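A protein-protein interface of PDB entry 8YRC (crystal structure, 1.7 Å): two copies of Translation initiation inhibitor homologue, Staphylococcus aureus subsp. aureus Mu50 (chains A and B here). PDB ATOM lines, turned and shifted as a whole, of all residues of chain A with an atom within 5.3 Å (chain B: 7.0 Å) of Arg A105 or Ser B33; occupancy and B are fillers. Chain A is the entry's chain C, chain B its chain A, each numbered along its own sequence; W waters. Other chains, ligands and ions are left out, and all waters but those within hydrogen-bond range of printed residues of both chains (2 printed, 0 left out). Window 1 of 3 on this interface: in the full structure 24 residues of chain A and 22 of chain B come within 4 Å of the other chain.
The backbone NH of Ser A106 is in hydrogen-bond range of the backbone carbonyl oxygen of Ala A77. The backbone carbonyl oxygen of Ile A79 sits close to the side-chain sulfur of Cys A107, at 3.8 Å. O of His B22 is in hydrogen-bond range of N of Ser B33 (2.9 Å). The backbone NH (N) of Ala A77 sits at hydrogen-bond distance from the backbone carbonyl oxygen (O) of Ala A104, at 2.9 Å. OD1 of Asn A91 is in hydrogen-bond range of NH1 of Arg A105, at 2.8 Å. O of Leu B123 is in hydrogen-bond range of N of Thr B32 (3.0 Å).
Printed residues of chain B that touch a printed residue of chain A: Pro B19, Tyr B20, Ser B21, Thr B24, Tyr B31, Thr B32, Ser B33, Gly B34, Glu B120 and Glu B122. Hydrophobic or aromatic side chains of chain B that line the printed part of chain A: Pro B19, Tyr B20 and Tyr B31. Printed residues of chain A that touch a printed residue of chain B: Lys A76, Asn A91, Tyr A94, Pro A103, Ala A104, Arg A105, Ser A106 and Cys A107.
N of Gly B34 lies within hydrogen-bond range of OG of Ser A106, 2.8 Å away. The backbone carbonyl oxygen (O) of Pro A103 lies within hydrogen-bond range of the backbone NH (N) of Ser B21, 3.2 Å away. N of Gly B34 lies within hydrogen-bond range of O of Arg A105 (3.3 Å). OE1 of Glu B122 lies within salt-bridge range of NZ of Lys A76. N of Arg A105 sits at hydrogen-bond distance from OG of Ser B33 (2.9 Å). OE1 of Glu B122 lies within hydrogen-bond range of OG of Ser A106 (2.5 Å).
No position is printed for both chains.
Water W1 lies within hydrogen-bond range of OE2 of Glu B120 (2.5 Å) and N of Cys A107 (2.8 Å). Water W2 lies within hydrogen-bond range of the backbone carbonyl oxygen of Pro B19, the side-chain hydroxyl of Tyr A94 and the backbone carbonyl oxygen of Pro A103.
Arg A105 touches just these residues of chain B: Pro B19 (3.7 Å), Tyr B20 (3.5 Å), Ser B33 (2.9 Å) and Gly B34 (3.3 Å). Of chain A, only Ala A104, Arg A105 and Ser A106 come within 4 Å of Ser B33. Printed residues of chain A within 4 Å of Tyr B20: Pro A103 and Arg A105. Of the printed residues of chain B, Tyr A94 touches Pro B19. Ala A77 touches none of the printed residues of chain B. The nearest residue of chain B that does not touch Arg A105 is Ser B21 (4.5 Å).
Among the printed residues, pairs that only touch across the chains: Lys A76 with Thr B32, Ala A104 with Tyr B31, Ala A104 with Ser B33, Pro A103 with Tyr B20, Asn A91 with Pro B19, Tyr A94 with Pro B19, Arg A105 with Tyr B20, Ala A104 with Thr B24, Arg A105 with Pro B19, Ala A104 with Ser B21, Ser A106 with Ser B33, Cys A107 with Glu B120, Ala A104 with Thr B32, Pro A103 with Thr B24, Lys A76 with Tyr B31 and Ser A106 with Glu B120.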
ATOM      1  N   LYS A  76     -22.800  18.910   5.502  1.00  0.00           N
ATOM      2  CA  LYS A  76     -22.768  17.551   4.917  1.00  0.00           C
ATOM      3  C   LYS A  76     -21.544  16.823   5.433  1.00  0.00           C
ATOM      4  O   LYS A  76     -20.430  17.337   5.351  1.00  0.00           O
ATOM      5  CB  LYS A  76     -22.803  17.591   3.384  1.00  0.00           C
ATOM      6  CG  LYS A  76     -22.483  16.277   2.675  1.00  0.00           C
ATOM      7  CD  LYS A  76     -23.598  15.320   2.888  1.00  0.00           C
ATOM      8  CE  LYS A  76     -23.716  14.267   1.808  1.00  0.00           C
ATOM      9  NZ  LYS A  76     -22.550  13.383   1.761  1.00  0.00           N
ATOM     10  N   ALA A  77     -21.760  15.588   5.839  1.00  0.00           N
ATOM     11  CA  ALA A  77     -20.682  14.717   6.319  1.00  0.00           C
ATOM     12  C   ALA A  77     -20.711  13.448   5.476  1.00  0.00           C
ATOM     13  O   ALA A  77     -21.769  12.950   5.187  1.00  0.00           O
ATOM     14  CB  ALA A  77     -20.861  14.437   7.781  1.00  0.00           C
ATOM     15  N   ILE A  79     -19.092   9.625   5.783  1.00  0.00           N
ATOM     16  CA  ILE A  79     -18.437   8.664   6.676  1.00  0.00           C
ATOM     17  C   ILE A  79     -18.156   7.402   5.852  1.00  0.00           C
ATOM     18  O   ILE A  79     -19.104   6.635   5.395  1.00  0.00           O
ATOM     19  CB  ILE A  79     -19.258   8.332   7.935  1.00  0.00           C
ATOM     20  CG1 ILE A  79     -19.834   9.564   8.641  1.00  0.00           C
ATOM     21  CG2 ILE A  79     -18.473   7.453   8.830  1.00  0.00           C
ATOM     22  CD1 ILE A  79     -20.599   9.262   9.932  1.00  0.00           C
ATOM     23  N   PHE A  87     -21.493   0.293  12.797  1.00  0.00           N
ATOM     24  CA  PHE A  87     -22.292   1.523  12.563  1.00  0.00           C
ATOM     25  C   PHE A  87     -22.867   2.062  13.874  1.00  0.00           C
ATOM     26  O   PHE A  87     -22.793   3.263  14.136  1.00  0.00           O
ATOM     27  CB  PHE A  87     -23.376   1.296  11.506  1.00  0.00           C
ATOM     28  CG  PHE A  87     -24.178   2.553  11.349  1.00  0.00           C
ATOM     29  CD1 PHE A  87     -23.595   3.671  10.768  1.00  0.00           C
ATOM     30  CD2 PHE A  87     -25.402   2.690  11.990  1.00  0.00           C
ATOM     31  CE1 PHE A  87     -24.280   4.879  10.705  1.00  0.00           C
ATOM     32  CE2 PHE A  87     -26.102   3.880  11.904  1.00  0.00           C
ATOM     33  CZ  PHE A  87     -25.541   4.967  11.263  1.00  0.00           C
ATOM     34  N   ASN A  91     -21.985   5.716  15.329  1.00  0.00           N
ATOM     35  CA  ASN A  91     -23.103   6.668  15.464  1.00  0.00           C
ATOM     36  C   ASN A  91     -23.211   7.315  16.858  1.00  0.00           C
ATOM     37  O   ASN A  91     -23.488   8.522  16.988  1.00  0.00           O
ATOM     38  CB  ASN A  91     -24.398   5.900  15.210  1.00  0.00           C
ATOM     39  CG  ASN A  91     -25.392   6.720  14.433  1.00  0.00           C
ATOM     40  OD1 ASN A  91     -25.040   7.698  13.777  1.00  0.00           O
ATOM     41  ND2 ASN A  91     -26.641   6.304  14.502  1.00  0.00           N
ATOM     42  N   TYR A  94     -20.463   9.813  16.998  1.00  0.00           N
ATOM     43  CA  TYR A  94     -20.859  10.865  16.047  1.00  0.00           C
ATOM     44  C   TYR A  94     -21.912  11.791  16.673  1.00  0.00           C
ATOM     45  O   TYR A  94     -21.802  13.016  16.545  1.00  0.00           O
ATOM     46  CB  TYR A  94     -21.355  10.216  14.779  1.00  0.00           C
ATOM     47  CG  TYR A  94     -21.653  11.170  13.675  1.00  0.00           C
ATOM     48  CD1 TYR A  94     -22.889  11.745  13.522  1.00  0.00           C
ATOM     49  CD2 TYR A  94     -20.650  11.535  12.791  1.00  0.00           C
ATOM     50  CE1 TYR A  94     -23.164  12.584  12.449  1.00  0.00           C
ATOM     51  CE2 TYR A  94     -20.895  12.382  11.725  1.00  0.00           C
ATOM     52  CZ  TYR A  94     -22.168  12.914  11.550  1.00  0.00           C
ATOM     53  OH  TYR A  94     -22.514  13.746  10.528  1.00  0.00           O
ATOM     54  N   PRO A 103     -26.530  17.620  10.508  1.00  0.00           N
ATOM     55  CA  PRO A 103     -26.404  17.851   9.090  1.00  0.00           C
ATOM     56  C   PRO A 103     -26.733  16.651   8.191  1.00  0.00           C
ATOM     57  O   PRO A 103     -26.961  15.606   8.648  1.00  0.00           O
ATOM     58  CB  PRO A 103     -24.932  18.248   8.950  1.00  0.00           C
ATOM     59  CG  PRO A 103     -24.247  17.637  10.104  1.00  0.00           C
ATOM     60  CD  PRO A 103     -25.276  17.500  11.195  1.00  0.00           C
ATOM     61  N   ALA A 104     -26.679  16.872   6.883  1.00  0.00           N
ATOM     62  CA  ALA A 104     -26.847  15.776   5.916  1.00  0.00           C
ATOM     63  C   ALA A 104     -25.656  14.814   6.060  1.00  0.00           C
ATOM     64  O   ALA A 104     -24.555  15.244   6.363  1.00  0.00           O
ATOM     65  CB  ALA A 104     -26.961  16.332   4.533  1.00  0.00           C
ATOM     66  N   ARG A 105     -25.876  13.542   5.779  1.00  0.00           N
ATOM     67  CA  ARG A 105     -24.816  12.532   5.977  1.00  0.00           C
ATOM     68  C   ARG A 105     -25.028  11.398   4.973  1.00  0.00           C
ATOM     69  O   ARG A 105     -26.158  11.036   4.656  1.00  0.00           O
ATOM     70  CB  ARG A 105     -24.885  12.022   7.426  1.00  0.00           C
ATOM     71  CG  ARG A 105     -23.704  11.205   7.918  1.00  0.00           C
ATOM     72  CD  ARG A 105     -23.987  10.700   9.318  1.00  0.00           C
ATOM     73  NE  ARG A 105     -24.976   9.638   9.408  1.00  0.00           N
ATOM     74  CZ  ARG A 105     -25.322   9.068  10.567  1.00  0.00           C
ATOM     75  NH1 ARG A 105     -24.725   9.464  11.689  1.00  0.00           N
ATOM     76  NH2 ARG A 105     -26.279   8.152  10.625  1.00  0.00           N
ATOM     77  N   SER A 106     -23.937  10.803   4.521  1.00  0.00           N
ATOM     78  CA  SER A 106     -23.898   9.476   3.873  1.00  0.00           C
ATOM     79  C   SER A 106     -22.862   8.630   4.609  1.00  0.00           C
ATOM     80  O   SER A 106     -21.863   9.203   5.056  1.00  0.00           O
ATOM     81  CB  SER A 106     -23.646   9.545   2.426  1.00  0.00           C
ATOM     82  OG  SER A 106     -24.617  10.357   1.757  1.00  0.00           O
ATOM     83  N   CYS A 107     -23.151   7.343   4.800  1.00  0.00           N
ATOM     84  CA  CYS A 107     -22.254   6.384   5.438  1.00  0.00           C
ATOM     85  C   CYS A 107     -22.244   5.101   4.597  1.00  0.00           C
ATOM     86  O   CYS A 107     -23.300   4.525   4.377  1.00  0.00           O
ATOM     87  CB  CYS A 107     -22.656   6.186   6.890  1.00  0.00           C
ATOM     88  SG  CYS A 107     -21.600   4.991   7.741  1.00  0.00           S
ATOM     89  N   ALA B  16     -34.720  10.070   9.007  1.00  0.00           N
ATOM     90  CA  ALA B  16     -33.279  10.029   9.342  1.00  0.00           C
ATOM     91  C   ALA B  16     -33.145   9.783  10.846  1.00  0.00           C
ATOM     92  O   ALA B  16     -33.152  10.780  11.604  1.00  0.00           O
ATOM     93  CB  ALA B  16     -32.614  11.311   8.933  1.00  0.00           C
ATOM     94  N   LEU B  17     -33.080   8.524  11.293  1.00  0.00           N
ATOM     95  CA  LEU B  17     -32.935   8.241  12.744  1.00  0.00           C
ATOM     96  C   LEU B  17     -31.582   8.766  13.258  1.00  0.00           C
ATOM     97  O   LEU B  17     -30.552   8.697  12.540  1.00  0.00           O
ATOM     98  CB  LEU B  17     -33.097   6.745  13.022  1.00  0.00           C
ATOM     99  CG  LEU B  17     -34.481   6.166  12.716  1.00  0.00           C
ATOM    100  CD1 LEU B  17     -34.478   4.642  12.863  1.00  0.00           C
ATOM    101  CD2 LEU B  17     -35.548   6.798  13.595  1.00  0.00           C
ATOM    102  N   GLY B  18     -31.605   9.290  14.475  1.00  0.00           N
ATOM    103  CA  GLY B  18     -30.417   9.797  15.178  1.00  0.00           C
ATOM    104  C   GLY B  18     -29.813  11.033  14.522  1.00  0.00           C
ATOM    105  O   GLY B  18     -30.502  11.926  14.000  1.00  0.00           O
ATOM    106  N   PRO B  19     -28.468  11.165  14.589  1.00  0.00           N
ATOM    107  CA  PRO B  19     -27.860  12.478  14.366  1.00  0.00           C
ATOM    108  C   PRO B  19     -27.613  12.952  12.913  1.00  0.00           C
ATOM    109  O   PRO B  19     -26.531  13.468  12.638  1.00  0.00           O
ATOM    110  CB  PRO B  19     -26.541  12.236  15.088  1.00  0.00           C
ATOM    111  CG  PRO B  19     -26.192  10.812  14.792  1.00  0.00           C
ATOM    112  CD  PRO B  19     -27.520  10.070  14.864  1.00  0.00           C
ATOM    113  N   TYR B  20     -28.599  12.858  12.041  1.00  0.00           N
ATOM    114  CA  TYR B  20     -28.509  13.411  10.678  1.00  0.00           C
ATOM    115  C   TYR B  20     -29.910  13.769  10.206  1.00  0.00           C
ATOM    116  O   TYR B  20     -30.883  13.410  10.905  1.00  0.00           O
ATOM    117  CB  TYR B  20     -27.767  12.454   9.756  1.00  0.00           C
ATOM    118  CG  TYR B  20     -28.554  11.272   9.250  1.00  0.00           C
ATOM    119  CD1 TYR B  20     -28.989  10.297  10.132  1.00  0.00           C
ATOM    120  CD2 TYR B  20     -28.920  11.179   7.922  1.00  0.00           C
ATOM    121  CE1 TYR B  20     -29.658   9.163   9.673  1.00  0.00           C
ATOM    122  CE2 TYR B  20     -29.614  10.074   7.454  1.00  0.00           C
ATOM    123  CZ  TYR B  20     -29.979   9.068   8.327  1.00  0.00           C
ATOM    124  OH  TYR B  20     -30.654   7.973   7.850  1.00  0.00           O
ATOM    125  N   SER B  21     -29.984  14.510   9.104  1.00  0.00           N
ATOM    126  CA  SER B  21     -31.219  15.053   8.523  1.00  0.00           C
ATOM    127  C   SER B  21     -31.280  14.678   7.056  1.00  0.00           C
ATOM    128  O   SER B  21     -30.241  14.392   6.481  1.00  0.00           O
ATOM    129  CB  SER B  21     -31.274  16.568   8.704  1.00  0.00           C
ATOM    130  OG  SER B  21     -31.207  16.886  10.090  1.00  0.00           O
ATOM    131  N   HIS B  22     -32.460  14.757   6.467  1.00  0.00           N
ATOM    132  CA  HIS B  22     -32.702  14.480   5.044  1.00  0.00           C
ATOM    133  C   HIS B  22     -31.816  15.306   4.144  1.00  0.00           C
ATOM    134  O   HIS B  22     -31.296  14.757   3.127  1.00  0.00           O
ATOM    135  CB  HIS B  22     -34.223  14.569   4.784  1.00  0.00           C
ATOM    136  CG  HIS B  22     -35.007  13.466   5.401  1.00  0.00           C
ATOM    137  ND1 HIS B  22     -36.299  13.668   5.877  1.00  0.00           N
ATOM    138  CD2 HIS B  22     -34.741  12.142   5.601  1.00  0.00           C
ATOM    139  CE1 HIS B  22     -36.821  12.515   6.257  1.00  0.00           C
ATOM    140  NE2 HIS B  22     -35.877  11.546   6.140  1.00  0.00           N
ATOM    141  N   ALA B  23     -31.617  16.588   4.461  1.00  0.00           N
ATOM    142  CA  ALA B  23     -30.799  17.491   3.644  1.00  0.00           C
ATOM    143  C   ALA B  23     -30.489  18.771   4.436  1.00  0.00           C
ATOM    144  O   ALA B  23     -31.087  19.015   5.516  1.00  0.00           O
ATOM    145  CB  ALA B  23     -31.472  17.750   2.307  1.00  0.00           C
ATOM    146  N   THR B  24     -29.501  19.518   3.973  1.00  0.00           N
ATOM    147  CA  THR B  24     -29.292  20.914   4.395  1.00  0.00           C
ATOM    148  C   THR B  24     -29.354  21.813   3.174  1.00  0.00           C
ATOM    149  O   THR B  24     -29.141  21.349   2.030  1.00  0.00           O
ATOM    150  CB  THR B  24     -27.969  21.081   5.161  1.00  0.00           C
ATOM    151  OG1 THR B  24     -26.877  20.716   4.323  1.00  0.00           O
ATOM    152  CG2 THR B  24     -27.906  20.308   6.473  1.00  0.00           C
ATOM    153  N   TYR B  31     -27.702  19.924  -0.100  1.00  0.00           N
ATOM    154  CA  TYR B  31     -26.826  18.746   0.136  1.00  0.00           C
ATOM    155  C   TYR B  31     -27.737  17.669   0.718  1.00  0.00           C
ATOM    156  O   TYR B  31     -28.164  17.869   1.844  1.00  0.00           O
ATOM    157  CB  TYR B  31     -25.695  19.066   1.088  1.00  0.00           C
ATOM    158  CG  TYR B  31     -24.765  20.150   0.605  1.00  0.00           C
ATOM    159  CD1 TYR B  31     -25.049  21.500   0.796  1.00  0.00           C
ATOM    160  CD2 TYR B  31     -23.647  19.851  -0.133  1.00  0.00           C
ATOM    161  CE1 TYR B  31     -24.211  22.507   0.339  1.00  0.00           C
ATOM    162  CE2 TYR B  31     -22.815  20.849  -0.617  1.00  0.00           C
ATOM    163  CZ  TYR B  31     -23.099  22.183  -0.413  1.00  0.00           C
ATOM    164  OH  TYR B  31     -22.257  23.159  -0.900  1.00  0.00           O
ATOM    165  N   THR B  32     -28.095  16.662  -0.051  1.00  0.00           N
ATOM    166  CA  THR B  32     -28.938  15.579   0.466  1.00  0.00           C
ATOM    167  C   THR B  32     -28.072  14.608   1.258  1.00  0.00           C
ATOM    168  O   THR B  32     -26.902  14.322   0.912  1.00  0.00           O
ATOM    169  CB  THR B  32     -29.833  14.848  -0.544  1.00  0.00           C
ATOM    170  OG1 THR B  32     -29.046  13.916  -1.272  1.00  0.00           O
ATOM    171  CG2 THR B  32     -30.569  15.757  -1.514  1.00  0.00           C
ATOM    172  N   SER B  33     -28.701  13.942   2.197  1.00  0.00           N
ATOM    173  CA  SER B  33     -28.179  12.651   2.708  1.00  0.00           C
ATOM    174  C   SER B  33     -28.222  11.618   1.569  1.00  0.00           C
ATOM    175  O   SER B  33     -29.097  11.743   0.674  1.00  0.00           O
ATOM    176  CB  SER B  33     -28.966  12.277   3.879  1.00  0.00           C
ATOM    177  OG  SER B  33     -28.605  13.086   4.968  1.00  0.00           O
ATOM    178  N   GLY B  34     -27.402  10.575   1.612  1.00  0.00           N
ATOM    179  CA  GLY B  34     -27.639   9.382   0.783  1.00  0.00           C
ATOM    180  C   GLY B  34     -29.021   8.809   1.052  1.00  0.00           C
ATOM    181  O   GLY B  34     -29.354   8.572   2.240  1.00  0.00           O
ATOM    182  N   GLN B  35     -29.841   8.620   0.024  1.00  0.00           N
ATOM    183  CA  GLN B  35     -31.129   7.906   0.146  1.00  0.00           C
ATOM    184  C   GLN B  35     -30.935   6.409  -0.150  1.00  0.00           C
ATOM    185  O   GLN B  35     -30.185   6.068  -1.047  1.00  0.00           O
ATOM    186  CB  GLN B  35     -32.193   8.517  -0.764  1.00  0.00           C
ATOM    187  CG  GLN B  35     -32.897   9.746  -0.197  1.00  0.00           C
ATOM    188  CD  GLN B  35     -33.725   9.394   1.021  1.00  0.00           C
ATOM    189  OE1 GLN B  35     -34.287   8.302   1.087  1.00  0.00           O
ATOM    190  NE2 GLN B  35     -33.674  10.241   2.041  1.00  0.00           N
ATOM    191  N   ILE B  36     -31.630   5.590   0.631  1.00  0.00           N
ATOM    192  CA  ILE B  36     -31.640   4.109   0.467  1.00  0.00           C
ATOM    193  C   ILE B  36     -33.108   3.735   0.285  1.00  0.00           C
ATOM    194  O   ILE B  36     -34.015   4.547   0.532  1.00  0.00           O
ATOM    195  CB  ILE B  36     -30.923   3.418   1.633  1.00  0.00           C
ATOM    196  CG1 ILE B  36     -31.499   3.836   2.996  1.00  0.00           C
ATOM    197  CG2 ILE B  36     -29.410   3.721   1.540  1.00  0.00           C
ATOM    198  CD1 ILE B  36     -31.251   2.859   4.127  1.00  0.00           C
ATOM    199  N   LEU B  60     -35.554  10.921  -3.335  1.00  0.00           N
ATOM    200  CA  LEU B  60     -34.750  12.123  -3.613  1.00  0.00           C
ATOM    201  C   LEU B  60     -35.639  13.204  -4.242  1.00  0.00           C
ATOM    202  O   LEU B  60     -35.486  14.377  -3.864  1.00  0.00           O
ATOM    203  CB  LEU B  60     -33.505  11.792  -4.437  1.00  0.00           C
ATOM    204  CG  LEU B  60     -32.398  11.106  -3.620  1.00  0.00           C
ATOM    205  CD1 LEU B  60     -31.465  10.344  -4.592  1.00  0.00           C
ATOM    206  CD2 LEU B  60     -31.627  12.049  -2.700  1.00  0.00           C
ATOM    207  N   VAL B  63     -37.159  14.843  -1.242  1.00  0.00           N
ATOM    208  CA  VAL B  63     -36.133  15.674  -0.530  1.00  0.00           C
ATOM    209  C   VAL B  63     -35.952  17.031  -1.233  1.00  0.00           C
ATOM    210  O   VAL B  63     -35.923  18.087  -0.568  1.00  0.00           O
ATOM    211  CB  VAL B  63     -34.776  14.946  -0.474  1.00  0.00           C
ATOM    212  CG1 VAL B  63     -33.731  15.864   0.137  1.00  0.00           C
ATOM    213  CG2 VAL B  63     -34.865  13.680   0.316  1.00  0.00           C
ATOM    214  N   GLU B 120     -27.457   3.338  -3.215  1.00  0.00           N
ATOM    215  CA  GLU B 120     -27.605   4.510  -2.311  1.00  0.00           C
ATOM    216  C   GLU B 120     -27.157   5.743  -3.098  1.00  0.00           C
ATOM    217  O   GLU B 120     -26.007   5.743  -3.578  1.00  0.00           O
ATOM    218  CB  GLU B 120     -26.764   4.321  -1.047  1.00  0.00           C
ATOM    219  CG  GLU B 120     -26.516   5.611  -0.287  1.00  0.00           C
ATOM    220  CD  GLU B 120     -26.148   5.424   1.175  1.00  0.00           C
ATOM    221  OE1 GLU B 120     -25.930   4.266   1.585  1.00  0.00           O
ATOM    222  OE2 GLU B 120     -26.081   6.435   1.900  1.00  0.00           O
ATOM    223  N   ILE B 121     -28.025   6.751  -3.228  1.00  0.00           N
ATOM    224  CA  ILE B 121     -27.649   7.931  -4.044  1.00  0.00           C
ATOM    225  C   ILE B 121     -27.775   9.209  -3.218  1.00  0.00           C
ATOM    226  O   ILE B 121     -28.737   9.363  -2.545  1.00  0.00           O
ATOM    227  CB  ILE B 121     -28.491   8.011  -5.333  1.00  0.00           C
ATOM    228  CG1 ILE B 121     -28.300   6.786  -6.216  1.00  0.00           C
ATOM    229  CG2 ILE B 121     -28.199   9.286  -6.087  1.00  0.00           C
ATOM    230  CD1 ILE B 121     -29.285   6.670  -7.321  1.00  0.00           C
ATOM    231  N   GLU B 122     -26.743  10.030  -3.281  1.00  0.00           N
ATOM    232  CA  GLU B 122     -26.723  11.401  -2.700  1.00  0.00           C
ATOM    233  C   GLU B 122     -26.615  12.425  -3.828  1.00  0.00           C
ATOM    234  O   GLU B 122     -25.978  12.158  -4.835  1.00  0.00           O
ATOM    235  CB  GLU B 122     -25.614  11.667  -1.680  1.00  0.00           C
ATOM    236  CG  GLU B 122     -24.212  11.379  -2.188  1.00  0.00           C
ATOM    237  CD  GLU B 122     -23.086  11.725  -1.235  1.00  0.00           C
ATOM    238  OE1 GLU B 122     -23.207  11.470  -0.052  1.00  0.00           O
ATOM    239  OE2 GLU B 122     -22.119  12.276  -1.712  1.00  0.00           O
ATOM    240  N   LEU B 123     -27.218  13.603  -3.622  1.00  0.00           N
ATOM    241  CA  LEU B 123     -27.269  14.721  -4.605  1.00  0.00           C
ATOM    242  C   LEU B 123     -26.745  16.008  -3.985  1.00  0.00           C
ATOM    243  O   LEU B 123     -26.973  16.280  -2.760  1.00  0.00           O
ATOM    244  CB  LEU B 123     -28.693  14.922  -5.135  1.00  0.00           C
ATOM    245  CG  LEU B 123     -29.418  13.689  -5.661  1.00  0.00           C
ATOM    246  CD1 LEU B 123     -30.871  14.048  -5.943  1.00  0.00           C
ATOM    247  CD2 LEU B 123     -28.768  13.133  -6.901  1.00  0.00           C
HETATM  248  O   HOH W   1     -25.658   6.205   4.336  1.00  0.00           O
HETATM  249  O   HOH W   2     -25.197  14.224  10.436  1.00  0.00           O
